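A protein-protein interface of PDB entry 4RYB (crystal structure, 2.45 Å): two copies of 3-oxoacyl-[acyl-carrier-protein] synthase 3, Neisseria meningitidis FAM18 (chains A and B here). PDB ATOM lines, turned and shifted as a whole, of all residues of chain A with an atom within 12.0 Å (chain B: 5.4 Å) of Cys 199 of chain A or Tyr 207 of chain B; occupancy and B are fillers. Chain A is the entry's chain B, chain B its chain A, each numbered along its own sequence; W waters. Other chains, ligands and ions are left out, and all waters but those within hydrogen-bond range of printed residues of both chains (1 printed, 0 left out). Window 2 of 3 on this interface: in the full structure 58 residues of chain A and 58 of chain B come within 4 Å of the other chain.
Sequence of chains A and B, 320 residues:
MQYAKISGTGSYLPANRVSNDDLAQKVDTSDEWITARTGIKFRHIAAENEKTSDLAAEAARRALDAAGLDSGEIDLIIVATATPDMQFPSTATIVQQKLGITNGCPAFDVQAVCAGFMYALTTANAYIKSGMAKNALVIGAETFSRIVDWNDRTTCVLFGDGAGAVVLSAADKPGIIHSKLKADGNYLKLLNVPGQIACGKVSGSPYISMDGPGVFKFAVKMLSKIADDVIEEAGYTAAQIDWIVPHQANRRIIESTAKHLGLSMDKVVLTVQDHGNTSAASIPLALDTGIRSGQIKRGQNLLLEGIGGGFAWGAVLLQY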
ATOM      1  N   ASP A  85       4.990  33.966 -23.280  1.00  0.00           N
ATOM      2  CA  ASP A  85       6.245  33.762 -22.565  1.00  0.00           C
ATOM      3  C   ASP A  85       6.415  32.310 -22.139  1.00  0.00           C
ATOM      4  O   ASP A  85       7.502  31.748 -22.251  1.00  0.00           O
ATOM      5  CB  ASP A  85       6.308  34.659 -21.327  1.00  0.00           C
ATOM      6  CG  ASP A  85       6.620  36.103 -21.663  1.00  0.00           C
ATOM      7  OD1 ASP A  85       6.205  36.577 -22.743  1.00  0.00           O
ATOM      8  OD2 ASP A  85       7.283  36.764 -20.836  1.00  0.00           O
ATOM      9  N   MET A  86       5.357  31.704 -21.648  1.00  0.00           N
ATOM     10  CA  MET A  86       5.349  30.370 -21.134  1.00  0.00           C
ATOM     11  C   MET A  86       4.161  29.519 -21.487  1.00  0.00           C
ATOM     12  O   MET A  86       3.148  30.019 -21.897  1.00  0.00           O
ATOM     13  CB  MET A  86       5.276  30.476 -19.635  1.00  0.00           C
ATOM     14  CG  MET A  86       6.436  31.085 -18.947  1.00  0.00           C
ATOM     15  SD  MET A  86       6.051  31.416 -17.264  1.00  0.00           S
ATOM     16  CE  MET A  86       7.490  32.303 -16.789  1.00  0.00           C
ATOM     17  N   GLN A  87       4.295  28.216 -21.307  1.00  0.00           N
ATOM     18  CA  GLN A  87       3.173  27.302 -21.471  1.00  0.00           C
ATOM     19  C   GLN A  87       2.029  27.813 -20.602  1.00  0.00           C
ATOM     20  O   GLN A  87       0.892  27.934 -21.060  1.00  0.00           O
ATOM     21  CB  GLN A  87       3.580  25.881 -21.080  1.00  0.00           C
ATOM     22  CG  GLN A  87       2.497  24.822 -21.249  1.00  0.00           C
ATOM     23  CD  GLN A  87       2.179  24.526 -22.698  1.00  0.00           C
ATOM     24  OE1 GLN A  87       3.060  24.545 -23.556  1.00  0.00           O
ATOM     25  NE2 GLN A  87       0.915  24.236 -22.978  1.00  0.00           N
ATOM     26  N   PHE A  88       2.353  28.117 -19.347  1.00  0.00           N
ATOM     27  CA  PHE A  88       1.475  28.888 -18.470  1.00  0.00           C
ATOM     28  C   PHE A  88       2.293  29.393 -17.273  1.00  0.00           C
ATOM     29  O   PHE A  88       3.382  28.881 -17.010  1.00  0.00           O
ATOM     30  CB  PHE A  88       0.248  28.054 -18.047  1.00  0.00           C
ATOM     31  CG  PHE A  88       0.514  27.025 -16.978  1.00  0.00           C
ATOM     32  CD1 PHE A  88       0.709  27.391 -15.654  1.00  0.00           C
ATOM     33  CD2 PHE A  88       0.503  25.677 -17.296  1.00  0.00           C
ATOM     34  CE1 PHE A  88       0.928  26.433 -14.680  1.00  0.00           C
ATOM     35  CE2 PHE A  88       0.716  24.718 -16.327  1.00  0.00           C
ATOM     36  CZ  PHE A  88       0.931  25.096 -15.017  1.00  0.00           C
ATOM     37  N   PRO A  89       1.788  30.411 -16.552  1.00  0.00           N
ATOM     38  CA  PRO A  89       0.494  31.090 -16.699  1.00  0.00           C
ATOM     39  C   PRO A  89       0.434  32.078 -17.864  1.00  0.00           C
ATOM     40  O   PRO A  89       1.367  32.158 -18.662  1.00  0.00           O
ATOM     41  CB  PRO A  89       0.345  31.829 -15.368  1.00  0.00           C
ATOM     42  CG  PRO A  89       1.736  32.121 -14.947  1.00  0.00           C
ATOM     43  CD  PRO A  89       2.574  30.970 -15.436  1.00  0.00           C
ATOM     44  N   GLY A 195       3.626  22.387 -33.752  1.00  0.00           N
ATOM     45  CA  GLY A 195       4.316  21.892 -32.574  1.00  0.00           C
ATOM     46  C   GLY A 195       3.675  22.231 -31.241  1.00  0.00           C
ATOM     47  O   GLY A 195       3.015  23.261 -31.092  1.00  0.00           O
ATOM     48  N   GLN A 196       3.875  21.345 -30.269  1.00  0.00           N
ATOM     49  CA  GLN A 196       3.449  21.581 -28.894  1.00  0.00           C
ATOM     50  C   GLN A 196       4.490  21.028 -27.931  1.00  0.00           C
ATOM     51  O   GLN A 196       5.276  20.149 -28.292  1.00  0.00           O
ATOM     52  CB  GLN A 196       2.089  20.933 -28.617  1.00  0.00           C
ATOM     53  CG  GLN A 196       2.156  19.428 -28.332  1.00  0.00           C
ATOM     54  CD  GLN A 196       0.796  18.788 -28.078  1.00  0.00           C
ATOM     55  OE1 GLN A 196       0.654  17.568 -28.167  1.00  0.00           O
ATOM     56  NE2 GLN A 196      -0.205  19.602 -27.751  1.00  0.00           N
ATOM     57  N   ILE A 197       4.484  21.536 -26.705  1.00  0.00           N
ATOM     58  CA  ILE A 197       5.329  20.994 -25.653  1.00  0.00           C
ATOM     59  C   ILE A 197       4.620  19.787 -25.046  1.00  0.00           C
ATOM     60  O   ILE A 197       3.545  19.916 -24.456  1.00  0.00           O
ATOM     61  CB  ILE A 197       5.635  22.047 -24.566  1.00  0.00           C
ATOM     62  CG1 ILE A 197       6.404  23.220 -25.182  1.00  0.00           C
ATOM     63  CG2 ILE A 197       6.428  21.420 -23.415  1.00  0.00           C
ATOM     64  CD1 ILE A 197       6.702  24.356 -24.220  1.00  0.00           C
ATOM     65  N   ALA A 198       5.222  18.613 -25.214  1.00  0.00           N
ATOM     66  CA  ALA A 198       4.651  17.370 -24.708  1.00  0.00           C
ATOM     67  C   ALA A 198       5.744  16.382 -24.314  1.00  0.00           C
ATOM     68  O   ALA A 198       6.660  16.112 -25.092  1.00  0.00           O
ATOM     69  CB  ALA A 198       3.734  16.751 -25.748  1.00  0.00           C
ATOM     70  N   CYS A 199       5.631  15.848 -23.101  1.00  0.00           N
ATOM     71  CA  CYS A 199       6.552  14.827 -22.605  1.00  0.00           C
ATOM     72  C   CYS A 199       8.004  15.293 -22.659  1.00  0.00           C
ATOM     73  O   CYS A 199       8.903  14.526 -23.008  1.00  0.00           O
ATOM     74  CB  CYS A 199       6.384  13.531 -23.403  1.00  0.00           C
ATOM     75  SG  CYS A 199       4.704  12.858 -23.349  1.00  0.00           S
ATOM     76  N   GLY A 200       8.222  16.556 -22.307  1.00  0.00           N
ATOM     77  CA  GLY A 200       9.562  17.089 -22.134  1.00  0.00           C
ATOM     78  C   GLY A 200      10.275  17.558 -23.390  1.00  0.00           C
ATOM     79  O   GLY A 200      11.453  17.912 -23.326  1.00  0.00           O
ATOM     80  N   LYS A 201       9.583  17.565 -24.526  1.00  0.00           N
ATOM     81  CA  LYS A 201      10.196  17.997 -25.780  1.00  0.00           C
ATOM     82  C   LYS A 201       9.153  18.614 -26.706  1.00  0.00           C
ATOM     83  O   LYS A 201       7.961  18.610 -26.397  1.00  0.00           O
ATOM     84  CB  LYS A 201      10.882  16.824 -26.484  1.00  0.00           C
ATOM     85  CG  LYS A 201       9.927  15.880 -27.203  1.00  0.00           C
ATOM     86  CD  LYS A 201      10.671  14.770 -27.924  1.00  0.00           C
ATOM     87  CE  LYS A 201       9.856  14.235 -29.095  1.00  0.00           C
ATOM     88  NZ  LYS A 201       8.396  14.151 -28.805  1.00  0.00           N
ATOM     89  N   VAL A 202       9.606  19.142 -27.841  1.00  0.00           N
ATOM     90  CA  VAL A 202       8.691  19.619 -28.872  1.00  0.00           C
ATOM     91  C   VAL A 202       8.114  18.436 -29.639  1.00  0.00           C
ATOM     92  O   VAL A 202       8.854  17.581 -30.123  1.00  0.00           O
ATOM     93  CB  VAL A 202       9.380  20.569 -29.879  1.00  0.00           C
ATOM     94  CG1 VAL A 202       8.379  21.069 -30.915  1.00  0.00           C
ATOM     95  CG2 VAL A 202      10.033  21.736 -29.168  1.00  0.00           C
ATOM     96  N   SER A 203       6.788  18.401 -29.741  1.00  0.00           N
ATOM     97  CA  SER A 203       6.093  17.378 -30.512  1.00  0.00           C
ATOM     98  C   SER A 203       5.445  18.016 -31.736  1.00  0.00           C
ATOM     99  O   SER A 203       4.464  18.748 -31.613  1.00  0.00           O
ATOM    100  CB  SER A 203       5.041  16.674 -29.655  1.00  0.00           C
ATOM    101  OG  SER A 203       4.370  15.667 -30.392  1.00  0.00           O
ATOM    102  N   GLY A 204       5.997  17.725 -32.911  1.00  0.00           N
ATOM    103  CA  GLY A 204       5.556  18.338 -34.154  1.00  0.00           C
ATOM    104  C   GLY A 204       6.476  19.472 -34.569  1.00  0.00           C
ATOM    105  O   GLY A 204       7.447  19.776 -33.875  1.00  0.00           O
ATOM    106  N   ARG B 146       0.853  15.496 -20.069  1.00  0.00           N
ATOM    107  CA  ARG B 146       1.956  15.660 -21.011  1.00  0.00           C
ATOM    108  C   ARG B 146       2.853  16.866 -20.711  1.00  0.00           C
ATOM    109  O   ARG B 146       3.800  17.130 -21.449  1.00  0.00           O
ATOM    110  CB  ARG B 146       1.400  15.758 -22.431  1.00  0.00           C
ATOM    111  CG  ARG B 146       0.544  14.556 -22.802  1.00  0.00           C
ATOM    112  CD  ARG B 146       0.401  14.394 -24.304  1.00  0.00           C
ATOM    113  NE  ARG B 146      -0.274  13.141 -24.639  1.00  0.00           N
ATOM    114  CZ  ARG B 146      -1.406  13.036 -25.332  1.00  0.00           C
ATOM    115  NH1 ARG B 146      -2.033  14.111 -25.803  1.00  0.00           N
ATOM    116  NH2 ARG B 146      -1.915  11.835 -25.564  1.00  0.00           N
ATOM    117  N   ILE B 147       2.555  17.587 -19.632  1.00  0.00           N
ATOM    118  CA  ILE B 147       3.432  18.654 -19.146  1.00  0.00           C
ATOM    119  C   ILE B 147       3.837  18.385 -17.696  1.00  0.00           C
ATOM    120  O   ILE B 147       4.338  19.270 -17.001  1.00  0.00           O
ATOM    121  CB  ILE B 147       2.763  20.045 -19.238  1.00  0.00           C
ATOM    122  CG1 ILE B 147       1.414  20.044 -18.514  1.00  0.00           C
ATOM    123  CG2 ILE B 147       2.593  20.452 -20.694  1.00  0.00           C
ATOM    124  CD1 ILE B 147       0.850  21.426 -18.272  1.00  0.00           C
ATOM    125  N   VAL B 148       3.604  17.155 -17.249  1.00  0.00           N
ATOM    126  CA  VAL B 148       4.024  16.708 -15.926  1.00  0.00           C
ATOM    127  C   VAL B 148       5.367  15.989 -15.990  1.00  0.00           C
ATOM    128  O   VAL B 148       5.627  15.222 -16.918  1.00  0.00           O
ATOM    129  CB  VAL B 148       2.961  15.778 -15.292  1.00  0.00           C
ATOM    130  CG1 VAL B 148       3.572  14.857 -14.242  1.00  0.00           C
ATOM    131  CG2 VAL B 148       1.822  16.590 -14.699  1.00  0.00           C
ATOM    132  N   ASP B 149       6.222  16.254 -15.007  1.00  0.00           N
ATOM    133  CA  ASP B 149       7.443  15.478 -14.832  1.00  0.00           C
ATOM    134  C   ASP B 149       7.127  14.242 -14.001  1.00  0.00           C
ATOM    135  O   ASP B 149       6.961  14.331 -12.786  1.00  0.00           O
ATOM    136  CB  ASP B 149       8.530  16.312 -14.151  1.00  0.00           C
ATOM    137  CG  ASP B 149       9.834  15.549 -13.978  1.00  0.00           C
ATOM    138  OD1 ASP B 149       9.995  14.473 -14.596  1.00  0.00           O
ATOM    139  OD2 ASP B 149      10.705  16.030 -13.223  1.00  0.00           O
ATOM    140  N   ASN B 192       3.848  27.190 -12.327  1.00  0.00           N
ATOM    141  CA  ASN B 192       4.136  27.547 -13.708  1.00  0.00           C
ATOM    142  C   ASN B 192       4.834  26.439 -14.484  1.00  0.00           C
ATOM    143  O   ASN B 192       5.435  25.535 -13.901  1.00  0.00           O
ATOM    144  CB  ASN B 192       4.998  28.812 -13.751  1.00  0.00           C
ATOM    145  CG  ASN B 192       6.321  28.643 -13.024  1.00  0.00           C
ATOM    146  OD1 ASN B 192       7.265  28.049 -13.550  1.00  0.00           O
ATOM    147  ND2 ASN B 192       6.396  29.168 -11.807  1.00  0.00           N
ATOM    148  N   VAL B 193       4.714  26.515 -15.807  1.00  0.00           N
ATOM    149  CA  VAL B 193       5.525  25.732 -16.733  1.00  0.00           C
ATOM    150  C   VAL B 193       6.386  26.721 -17.518  1.00  0.00           C
ATOM    151  O   VAL B 193       5.906  27.330 -18.473  1.00  0.00           O
ATOM    152  CB  VAL B 193       4.658  24.882 -17.693  1.00  0.00           C
ATOM    153  CG1 VAL B 193       5.520  24.233 -18.780  1.00  0.00           C
ATOM    154  CG2 VAL B 193       3.894  23.819 -16.933  1.00  0.00           C
ATOM    155  N   PRO B 194       7.659  26.893 -17.118  1.00  0.00           N
ATOM    156  CA  PRO B 194       8.484  27.973 -17.676  1.00  0.00           C
ATOM    157  C   PRO B 194       8.697  27.875 -19.183  1.00  0.00           C
ATOM    158  O   PRO B 194       8.838  28.899 -19.851  1.00  0.00           O
ATOM    159  CB  PRO B 194       9.825  27.810 -16.946  1.00  0.00           C
ATOM    160  CG  PRO B 194       9.540  26.966 -15.763  1.00  0.00           C
ATOM    161  CD  PRO B 194       8.417  26.075 -16.154  1.00  0.00           C
ATOM    162  N   SER B 205      12.098  24.971 -18.823  1.00  0.00           N
ATOM    163  CA  SER B 205      11.550  23.697 -18.372  1.00  0.00           C
ATOM    164  C   SER B 205      10.195  23.402 -19.019  1.00  0.00           C
ATOM    165  O   SER B 205       9.306  24.252 -19.001  1.00  0.00           O
ATOM    166  CB  SER B 205      11.405  23.690 -16.850  1.00  0.00           C
ATOM    167  OG  SER B 205      10.797  22.489 -16.408  1.00  0.00           O
ATOM    168  N   PRO B 206      10.033  22.194 -19.588  1.00  0.00           N
ATOM    169  CA  PRO B 206       8.758  21.799 -20.198  1.00  0.00           C
ATOM    170  C   PRO B 206       7.786  21.176 -19.198  1.00  0.00           C
ATOM    171  O   PRO B 206       6.724  20.697 -19.598  1.00  0.00           O
ATOM    172  CB  PRO B 206       9.183  20.768 -21.239  1.00  0.00           C
ATOM    173  CG  PRO B 206      10.366  20.112 -20.617  1.00  0.00           C
ATOM    174  CD  PRO B 206      11.079  21.183 -19.833  1.00  0.00           C
ATOM    175  N   TYR B 207       8.151  21.189 -17.918  1.00  0.00           N
ATOM    176  CA  TYR B 207       7.377  20.509 -16.882  1.00  0.00           C
ATOM    177  C   TYR B 207       6.814  21.486 -15.854  1.00  0.00           C
ATOM    178  O   TYR B 207       7.308  22.604 -15.709  1.00  0.00           O
ATOM    179  CB  TYR B 207       8.252  19.467 -16.183  1.00  0.00           C
ATOM    180  CG  TYR B 207       8.709  18.342 -17.088  1.00  0.00           C
ATOM    181  CD1 TYR B 207       7.800  17.642 -17.871  1.00  0.00           C
ATOM    182  CD2 TYR B 207      10.049  17.986 -17.163  1.00  0.00           C
ATOM    183  CE1 TYR B 207       8.212  16.614 -18.698  1.00  0.00           C
ATOM    184  CE2 TYR B 207      10.471  16.960 -17.987  1.00  0.00           C
ATOM    185  CZ  TYR B 207       9.548  16.279 -18.753  1.00  0.00           C
ATOM    186  OH  TYR B 207       9.958  15.256 -19.577  1.00  0.00           O
ATOM    187  N   ILE B 208       5.776  21.050 -15.143  1.00  0.00           N
ATOM    188  CA  ILE B 208       5.149  21.872 -14.115  1.00  0.00           C
ATOM    189  C   ILE B 208       6.047  22.023 -12.892  1.00  0.00           C
ATOM    190  O   ILE B 208       6.551  21.041 -12.345  1.00  0.00           O
ATOM    191  CB  ILE B 208       3.786  21.285 -13.677  1.00  0.00           C
ATOM    192  CG1 ILE B 208       2.783  21.363 -14.831  1.00  0.00           C
ATOM    193  CG2 ILE B 208       3.233  22.032 -12.463  1.00  0.00           C
ATOM    194  CD1 ILE B 208       1.511  20.563 -14.608  1.00  0.00           C
ATOM    195  N   SER B 209       6.238  23.275 -12.485  1.00  0.00           N
ATOM    196  CA  SER B 209       6.917  23.604 -11.240  1.00  0.00           C
ATOM    197  C   SER B 209       5.895  24.186 -10.279  1.00  0.00           C
ATOM    198  O   SER B 209       5.170  25.114 -10.631  1.00  0.00           O
ATOM    199  CB  SER B 209       8.052  24.597 -11.478  1.00  0.00           C
ATOM    200  OG  SER B 209       8.543  25.101 -10.247  1.00  0.00           O
HETATM  201  O   HOH W   1       6.390  18.534 -21.476  1.00  0.00           O
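Asp 85 of chain A touches Pro 194 of chain B. CB of Met 86 of chain A touches O of Val 193 of chain B, at 3.4 Å. Met 86 of chain A touches Pro 194 of chain B (CG to O, 3.4 Å). Ile 147 of chain B touches Phe 88 of chain A. Asn 192 of chain B touches Phe 88 of chain A (CA to CE1, 3.5 Å). CD of Pro 89 of chain A touches CB of Asn 192 of chain B, at 3.7 Å. Pro 206 of chain B touches Ile 197 of chain A. Arg 146 of chain B touches Ala 198 of chain A (O to CA, 3.4 Å). Tyr 207 of chain B touches Cys 199 of chain A. CA of Gly 200 of chain A touches CG of Pro 206 of chain B, at 3.5 Å.
No position is printed for both chains.
OG of Ser 205 of chain B lies close to N of Tyr 207 of chain B, at 3.3 Å. N of Ile 208 of chain B is in hydrogen-bond range of O of Ile 147 of chain B. The backbone carbonyl oxygen of Asn 192 of chain B sits at hydrogen-bond distance from the backbone NH of Ser 209 of chain B, 2.8 Å away.
Printed residues of chain B within 4 Å of Asp 85 of chain A: Pro 194 (3.96 Å). Of the printed residues of chain B, Gln 87 of chain A touches Val 193 (3.4 Å). Of the printed residues of chain B, Ile 197 of chain A touches Ile 147 (3.9 Å) and Pro 206 (3.6 Å). Cys 199 of chain A touches just these residues of chain B: Arg 146 (2.8 Å) and Tyr 207 (3.6 Å). Arg 146 of chain B touches just these residues of chain A: Ala 198 and Cys 199. No residue of chain A comes within 4 Å of Val 148 of chain B. No residue of chain A comes within 4 Å of Asp 149 of chain B. Of chain A, only Phe 88 and Pro 89 come within 4 Å of Asn 192 of chain B. Of the printed residues of chain A, Pro 194 of chain B touches Asp 85 (3.96 Å) and Met 86 (3.4 Å). No residue of chain A comes within 4 Å of Ser 205 of chain B. Pro 206 of chain B touches two residues of chain A. Of chain A, only Cys 199 and Gly 200 come within 4 Å of Tyr 207 of chain B.
Water W1 lies within hydrogen-bond range of N of Gly 200 of chain A, O of Pro 206 of chain B, O of Arg 146 of chain B and N of Cys 199 of chain A.
Hydrophobic or aromatic side chains of chain B within 4 Å of the printed part of chain A: Ile 147, Val 193, Pro 206 and Tyr 207. Along chain B the printed residues that touch a printed residue of chain A span positions 146 to 207. Among the printed residues, 15 pairs touch across the chains.
The side-chain hydroxyl (OH) of Tyr 207 of chain B lies close to the backbone NH (N) of Gly 200 of chain A (3.5 Å). O of Phe 88 of chain A sits at hydrogen-bond distance from N of Val 193 of chain B, 3.0 Å away. O of Arg 146 of chain B lies within hydrogen-bond range of N of Cys 199 of chain A (2.8 Å). O of Val 193 of chain B sits at hydrogen-bond distance from N of Gln 87 of chain A, 3.4 Å away.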
